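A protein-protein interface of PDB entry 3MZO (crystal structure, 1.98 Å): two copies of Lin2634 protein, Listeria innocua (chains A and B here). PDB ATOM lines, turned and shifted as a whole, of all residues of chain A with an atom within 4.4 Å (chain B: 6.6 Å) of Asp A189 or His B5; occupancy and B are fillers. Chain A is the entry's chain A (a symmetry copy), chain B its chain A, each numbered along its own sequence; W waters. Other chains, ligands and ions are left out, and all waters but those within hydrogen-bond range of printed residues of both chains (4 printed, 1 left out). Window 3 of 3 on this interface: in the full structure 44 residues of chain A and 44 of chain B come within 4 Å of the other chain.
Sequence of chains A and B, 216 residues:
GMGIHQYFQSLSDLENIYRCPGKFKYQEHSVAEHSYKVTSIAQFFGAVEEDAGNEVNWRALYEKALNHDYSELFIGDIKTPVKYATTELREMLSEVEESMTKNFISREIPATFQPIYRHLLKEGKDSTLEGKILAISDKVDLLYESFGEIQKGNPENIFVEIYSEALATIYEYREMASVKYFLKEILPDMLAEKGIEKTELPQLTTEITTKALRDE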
ATOM      1  N   TYR A 144     -14.603  -2.578   1.266  1.00  0.00           N
ATOM      2  CA  TYR A 144     -13.275  -2.950   1.737  1.00  0.00           C
ATOM      3  C   TYR A 144     -12.547  -3.854   0.778  1.00  0.00           C
ATOM      4  O   TYR A 144     -11.351  -3.660   0.558  1.00  0.00           O
ATOM      5  CB  TYR A 144     -13.332  -3.575   3.149  1.00  0.00           C
ATOM      6  CG  TYR A 144     -13.248  -2.487   4.171  1.00  0.00           C
ATOM      7  CD1 TYR A 144     -14.381  -1.723   4.503  1.00  0.00           C
ATOM      8  CD2 TYR A 144     -12.041  -2.177   4.770  1.00  0.00           C
ATOM      9  CE1 TYR A 144     -14.314  -0.698   5.432  1.00  0.00           C
ATOM     10  CE2 TYR A 144     -11.940  -1.106   5.677  1.00  0.00           C
ATOM     11  CZ  TYR A 144     -13.090  -0.386   6.013  1.00  0.00           C
ATOM     12  OH  TYR A 144     -13.038   0.655   6.893  1.00  0.00           O
ATOM     13  N   GLU A 185     -16.570   8.686  10.926  1.00  0.00           N
ATOM     14  CA  GLU A 185     -15.340   8.178  11.529  1.00  0.00           C
ATOM     15  C   GLU A 185     -14.540   7.177  10.686  1.00  0.00           C
ATOM     16  O   GLU A 185     -13.305   7.185  10.696  1.00  0.00           O
ATOM     17  CB  GLU A 185     -15.673   7.527  12.880  1.00  0.00           C
ATOM     18  CG  GLU A 185     -16.184   8.504  13.942  1.00  0.00           C
ATOM     19  CD  GLU A 185     -15.158   9.569  14.320  1.00  0.00           C
ATOM     20  OE1 GLU A 185     -13.949   9.369  14.111  1.00  0.00           O
ATOM     21  OE2 GLU A 185     -15.581  10.604  14.812  1.00  0.00           O
ATOM     22  N   ILE A 186     -15.235   6.332   9.939  1.00  0.00           N
ATOM     23  CA  ILE A 186     -14.593   5.209   9.262  1.00  0.00           C
ATOM     24  C   ILE A 186     -14.118   5.623   7.873  1.00  0.00           C
ATOM     25  O   ILE A 186     -12.943   5.508   7.574  1.00  0.00           O
ATOM     26  CB  ILE A 186     -15.540   4.011   9.198  1.00  0.00           C
ATOM     27  CG1 ILE A 186     -15.916   3.592  10.636  1.00  0.00           C
ATOM     28  CG2 ILE A 186     -14.865   2.809   8.491  1.00  0.00           C
ATOM     29  CD1 ILE A 186     -16.926   2.337  10.729  1.00  0.00           C
ATOM     30  N   LEU A 187     -15.032   6.166   7.070  1.00  0.00           N
ATOM     31  CA  LEU A 187     -14.725   6.543   5.699  1.00  0.00           C
ATOM     32  C   LEU A 187     -13.579   7.543   5.634  1.00  0.00           C
ATOM     33  O   LEU A 187     -12.723   7.421   4.751  1.00  0.00           O
ATOM     34  CB  LEU A 187     -15.961   7.067   4.956  1.00  0.00           C
ATOM     35  CG  LEU A 187     -15.822   7.461   3.456  1.00  0.00           C
ATOM     36  CD1 LEU A 187     -15.460   6.286   2.577  1.00  0.00           C
ATOM     37  CD2 LEU A 187     -17.149   8.050   2.982  1.00  0.00           C
ATOM     38  N   PRO A 188     -13.538   8.519   6.560  1.00  0.00           N
ATOM     39  CA  PRO A 188     -12.397   9.449   6.450  1.00  0.00           C
ATOM     40  C   PRO A 188     -11.044   8.774   6.690  1.00  0.00           C
ATOM     41  O   PRO A 188     -10.043   9.203   6.086  1.00  0.00           O
ATOM     42  CB  PRO A 188     -12.691  10.519   7.526  1.00  0.00           C
ATOM     43  CG  PRO A 188     -14.193  10.519   7.597  1.00  0.00           C
ATOM     44  CD  PRO A 188     -14.594   9.054   7.436  1.00  0.00           C
ATOM     45  N   ASP A 189     -11.010   7.734   7.526  1.00  0.00           N
ATOM     46  CA  ASP A 189      -9.771   6.990   7.780  1.00  0.00           C
ATOM     47  C   ASP A 189      -9.350   6.255   6.518  1.00  0.00           C
ATOM     48  O   ASP A 189      -8.169   6.227   6.185  1.00  0.00           O
ATOM     49  CB  ASP A 189      -9.902   5.993   8.930  1.00  0.00           C
ATOM     50  CG  ASP A 189      -9.852   6.675  10.309  1.00  0.00           C
ATOM     51  OD1 ASP A 189      -9.629   7.875  10.323  1.00  0.00           O
ATOM     52  OD2 ASP A 189     -10.100   6.038  11.342  1.00  0.00           O
ATOM     53  N   MET A 190     -10.328   5.673   5.829  1.00  0.00           N
ATOM     54  CA  MET A 190     -10.089   5.037   4.542  1.00  0.00           C
ATOM     55  C   MET A 190      -9.439   6.000   3.552  1.00  0.00           C
ATOM     56  O   MET A 190      -8.414   5.690   2.954  1.00  0.00           O
ATOM     57  CB  MET A 190     -11.382   4.507   3.913  1.00  0.00           C
ATOM     58  CG  MET A 190     -12.162   3.503   4.749  1.00  0.00           C
ATOM     59  SD  MET A 190     -13.688   2.779   3.759  1.00  0.00           S
ATOM     60  CE  MET A 190     -12.674   2.488   2.120  1.00  0.00           C
ATOM     61  N   LEU A 191     -10.039   7.175   3.393  1.00  0.00           N
ATOM     62  CA  LEU A 191      -9.596   8.129   2.401  1.00  0.00           C
ATOM     63  C   LEU A 191      -8.283   8.810   2.775  1.00  0.00           C
ATOM     64  O   LEU A 191      -7.630   9.348   1.904  1.00  0.00           O
ATOM     65  CB  LEU A 191     -10.690   9.174   2.122  1.00  0.00           C
ATOM     66  CG  LEU A 191     -11.940   8.603   1.434  1.00  0.00           C
ATOM     67  CD1 LEU A 191     -13.000   9.670   1.314  1.00  0.00           C
ATOM     68  CD2 LEU A 191     -11.599   8.007   0.071  1.00  0.00           C
ATOM     69  N   ALA A 192      -7.905   8.748   4.047  1.00  0.00           N
ATOM     70  CA  ALA A 192      -6.662   9.316   4.530  1.00  0.00           C
ATOM     71  C   ALA A 192      -5.510   8.348   4.352  1.00  0.00           C
ATOM     72  O   ALA A 192      -4.392   8.698   4.641  1.00  0.00           O
ATOM     73  CB  ALA A 192      -6.798   9.724   6.065  1.00  0.00           C
ATOM     74  N   GLU A 193      -5.760   7.117   3.919  1.00  0.00           N
ATOM     75  CA  GLU A 193      -4.662   6.178   3.704  1.00  0.00           C
ATOM     76  C   GLU A 193      -3.677   6.729   2.683  1.00  0.00           C
ATOM     77  O   GLU A 193      -4.083   7.429   1.777  1.00  0.00           O
ATOM     78  CB  GLU A 193      -5.214   4.853   3.208  1.00  0.00           C
ATOM     79  CG  GLU A 193      -6.011   4.104   4.271  1.00  0.00           C
ATOM     80  CD  GLU A 193      -5.165   3.276   5.182  1.00  0.00           C
ATOM     81  OE1 GLU A 193      -3.944   3.286   5.036  1.00  0.00           O
ATOM     82  OE2 GLU A 193      -5.724   2.602   6.059  1.00  0.00           O
ATOM     83  N   GLY B   1      -3.780   4.701  12.413  1.00  0.00           N
ATOM     84  CA  GLY B   1      -3.814   4.689  13.908  1.00  0.00           C
ATOM     85  C   GLY B   1      -5.129   4.129  14.442  1.00  0.00           C
ATOM     86  O   GLY B   1      -5.828   3.386  13.736  1.00  0.00           O
ATOM     87  N   MET B   2      -5.454   4.495  15.682  1.00  0.00           N
ATOM     88  CA  MET B   2      -6.693   4.082  16.366  1.00  0.00           C
ATOM     89  C   MET B   2      -7.977   4.338  15.548  1.00  0.00           C
ATOM     90  O   MET B   2      -8.278   5.463  15.192  1.00  0.00           O
ATOM     91  CB  MET B   2      -6.788   4.839  17.701  1.00  0.00           C
ATOM     92  CG  MET B   2      -7.899   4.393  18.671  1.00  0.00           C
ATOM     93  SD  MET B   2      -7.613   4.995  20.584  1.00  0.00           S
ATOM     94  CE  MET B   2      -5.734   4.487  20.791  1.00  0.00           C
ATOM     95  N   GLY B   3      -8.722   3.289  15.240  1.00  0.00           N
ATOM     96  CA  GLY B   3     -10.021   3.455  14.589  1.00  0.00           C
ATOM     97  C   GLY B   3     -10.630   2.133  14.160  1.00  0.00           C
ATOM     98  O   GLY B   3      -9.920   1.147  13.947  1.00  0.00           O
ATOM     99  N   ILE B   4     -11.955   2.118  14.024  1.00  0.00           N
ATOM    100  CA  ILE B   4     -12.680   0.961  13.570  1.00  0.00           C
ATOM    101  C   ILE B   4     -12.280   0.574  12.138  1.00  0.00           C
ATOM    102  O   ILE B   4     -12.296  -0.605  11.788  1.00  0.00           O
ATOM    103  CB  ILE B   4     -14.213   1.153  13.689  1.00  0.00           C
ATOM    104  CG1 ILE B   4     -14.603   1.430  15.159  1.00  0.00           C
ATOM    105  CG2 ILE B   4     -14.982  -0.100  13.226  1.00  0.00           C
ATOM    106  CD1 ILE B   4     -14.345   0.247  16.090  1.00  0.00           C
ATOM    107  N   HIS B   5     -11.857   1.551  11.344  1.00  0.00           N
ATOM    108  CA  HIS B   5     -11.349   1.264  10.001  1.00  0.00           C
ATOM    109  C   HIS B   5     -10.215   0.223  10.082  1.00  0.00           C
ATOM    110  O   HIS B   5     -10.195  -0.742   9.325  1.00  0.00           O
ATOM    111  CB  HIS B   5     -10.911   2.569   9.296  1.00  0.00           C
ATOM    112  CG  HIS B   5     -10.004   2.346   8.141  1.00  0.00           C
ATOM    113  ND1 HIS B   5     -10.432   1.747   6.976  1.00  0.00           N
ATOM    114  CD2 HIS B   5      -8.680   2.591   7.984  1.00  0.00           C
ATOM    115  CE1 HIS B   5      -9.405   1.641   6.145  1.00  0.00           C
ATOM    116  NE2 HIS B   5      -8.331   2.144   6.735  1.00  0.00           N
ATOM    117  N   GLN B   6      -9.309   0.399  11.028  1.00  0.00           N
ATOM    118  CA  GLN B   6      -8.190  -0.531  11.206  1.00  0.00           C
ATOM    119  C   GLN B   6      -8.692  -1.915  11.559  1.00  0.00           C
ATOM    120  O   GLN B   6      -8.134  -2.931  11.129  1.00  0.00           O
ATOM    121  CB  GLN B   6      -7.264  -0.058  12.352  1.00  0.00           C
ATOM    122  CG  GLN B   6      -6.334   1.048  11.976  1.00  0.00           C
ATOM    123  CD  GLN B   6      -5.166   0.556  11.130  1.00  0.00           C
ATOM    124  OE1 GLN B   6      -5.027   0.942   9.966  1.00  0.00           O
ATOM    125  NE2 GLN B   6      -4.331  -0.315  11.709  1.00  0.00           N
ATOM    126  N   TYR B   7      -9.706  -1.956  12.411  1.00  0.00           N
ATOM    127  CA  TYR B   7     -10.302  -3.224  12.815  1.00  0.00           C
ATOM    128  C   TYR B   7     -10.940  -3.923  11.607  1.00  0.00           C
ATOM    129  O   TYR B   7     -10.727  -5.126  11.399  1.00  0.00           O
ATOM    130  CB  TYR B   7     -11.315  -3.003  13.913  1.00  0.00           C
ATOM    131  CG  TYR B   7     -12.188  -4.193  14.156  1.00  0.00           C
ATOM    132  CD1 TYR B   7     -11.686  -5.338  14.756  1.00  0.00           C
ATOM    133  CD2 TYR B   7     -13.518  -4.171  13.807  1.00  0.00           C
ATOM    134  CE1 TYR B   7     -12.490  -6.452  14.978  1.00  0.00           C
ATOM    135  CE2 TYR B   7     -14.323  -5.296  13.972  1.00  0.00           C
ATOM    136  CZ  TYR B   7     -13.804  -6.437  14.565  1.00  0.00           C
ATOM    137  OH  TYR B   7     -14.631  -7.521  14.777  1.00  0.00           O
ATOM    138  N   PHE B   8     -11.726  -3.178  10.828  1.00  0.00           N
ATOM    139  CA  PHE B   8     -12.317  -3.730   9.624  1.00  0.00           C
ATOM    140  C   PHE B   8     -11.247  -4.287   8.640  1.00  0.00           C
ATOM    141  O   PHE B   8     -11.441  -5.372   8.070  1.00  0.00           O
ATOM    142  CB  PHE B   8     -13.189  -2.720   8.911  1.00  0.00           C
ATOM    143  CG  PHE B   8     -14.545  -2.460   9.567  1.00  0.00           C
ATOM    144  CD1 PHE B   8     -15.018  -3.218  10.654  1.00  0.00           C
ATOM    145  CD2 PHE B   8     -15.366  -1.477   9.043  1.00  0.00           C
ATOM    146  CE1 PHE B   8     -16.296  -2.977  11.186  1.00  0.00           C
ATOM    147  CE2 PHE B   8     -16.637  -1.251   9.556  1.00  0.00           C
ATOM    148  CZ  PHE B   8     -17.078  -1.978  10.655  1.00  0.00           C
ATOM    149  N   GLN B   9     -10.147  -3.556   8.427  1.00  0.00           N
ATOM    150  CA  GLN B   9      -9.050  -4.060   7.563  1.00  0.00           C
ATOM    151  C   GLN B   9      -8.485  -5.369   8.086  1.00  0.00           C
ATOM    152  O   GLN B   9      -8.235  -6.306   7.326  1.00  0.00           O
ATOM    153  CB  GLN B   9      -7.914  -3.059   7.452  1.00  0.00           C
ATOM    154  CG  GLN B   9      -8.226  -1.861   6.633  1.00  0.00           C
ATOM    155  CD  GLN B   9      -7.018  -0.963   6.482  1.00  0.00           C
ATOM    156  OE1 GLN B   9      -6.376  -0.535   7.476  1.00  0.00           O
ATOM    157  NE2 GLN B   9      -6.697  -0.670   5.249  1.00  0.00           N
ATOM    158  N   SER B  10      -8.346  -5.445   9.392  1.00  0.00           N
ATOM    159  CA  SER B  10      -7.803  -6.630  10.067  1.00  0.00           C
ATOM    160  C   SER B  10      -8.559  -7.922   9.824  1.00  0.00           C
ATOM    161  O   SER B  10      -7.955  -8.980   9.848  1.00  0.00           O
ATOM    162  CB  SER B  10      -7.652  -6.411  11.584  1.00  0.00           C
ATOM    163  OG  SER B  10      -8.842  -6.649  12.322  1.00  0.00           O
HETATM  164  O   HOH W   1      -9.829   7.106  13.702  1.00  0.00           O
HETATM  165  O   HOH W   2      -3.960   0.229   5.269  1.00  0.00           O
HETATM  166  O   HOH W   3      -8.216   3.733  11.543  1.00  0.00           O
HETATM  167  O   HOH W   4     -12.115   4.384  11.679  1.00  0.00           O
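The side-chain carboxylate (OE2) of Glu A193 is in hydrogen-bond range of a ring nitrogen (NE2) of His B5, at 2.7 Å.
OH of Tyr A144 sits at hydrogen-bond distance from ND1 of His B5 (2.8 Å).
CZ of Tyr A144 touches CB of Phe B8 (3.7 Å).
CE2 of Tyr A144 touches CG of Gln B9, 3.9 Å away.
Ile B4 touches Ile A186 (CG2 to CD1, 3.99 Å).
CB of His B5 touches O of Ile A186, 3.97 Å away.
Ile A186 touches Phe B8 (CD1 to CE2, 3.8 Å).
Asp A189 touches His B5 (CB to CB, 3.6 Å).
CG of Met A190 touches ND1 of His B5, 3.3 Å away.
Gln B9 touches Glu A193.
A ring nitrogen (NE2) of His B5 lies close to the side-chain amide oxygen (OE1) of Gln B9 (3.4 Å).
The side-chain amide oxygen (OE1) of Gln B6 lies close to the side-chain amide oxygen (OE1) of Gln B9 (3.2 Å).
Water W1 bridges the side-chain carboxylate (OD2) of Asp A189 (2.6 Å) and the backbone carbonyl oxygen (O) of Met B2 (2.7 Å).
Water W4 lies within hydrogen-bond range of OD2 of Asp A189, N of His B5, O of Glu A185 and N of Ile B4.
Water W2 lies within hydrogen-bond range of the side-chain amide nitrogen (NE2) of Gln B9 (2.9 Å) and the side-chain carboxylate (OE2) of Glu A193 (3.1 Å).
Water W3 lies within hydrogen-bond range of OD2 of Asp A189 (3.0 Å) and O of Gly B1 (3.3 Å).
Of chain B, only His B5 comes within 4 Å of Asp A189.
Printed residues of chain A within 4 Å of His B5: Tyr A144 (2.8 Å), Ile A186 (3.97 Å), Asp A189 (3.6 Å), Met A190 (3.3 Å) and Glu A193 (2.7 Å).
Printed residues of chain B within 4 Å of Ile A186: Ile B4 (3.99 Å), His B5 (3.97 Å) and Phe B8 (3.8 Å).
Of the printed residues of chain A, Ile B4 touches Ile A186 (3.99 Å).
Printed residues of chain B within 4 Å of Tyr A144: His B5 (2.8 Å), Phe B8 (3.7 Å) and Gln B9 (3.9 Å).
Tyr B7 touches none of the printed residues of chain A.
The nearest residue of chain B that does not touch Asp A189 is Gly B3 (4.1 Å).
The nearest printed residue of chain A that does not touch His B5 is Glu A185 (5.4 Å).
The nearest printed residue of chain A that does not touch Phe B8 is Met A190 (7.0 Å).
No position is printed for both chains.
Of the 10 pairs that touch across the chains among the printed residues, none has its exchanged pair printed and touching as well.
Of the 10 printed residues of chain A, 5 touch a printed residue of chain B.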
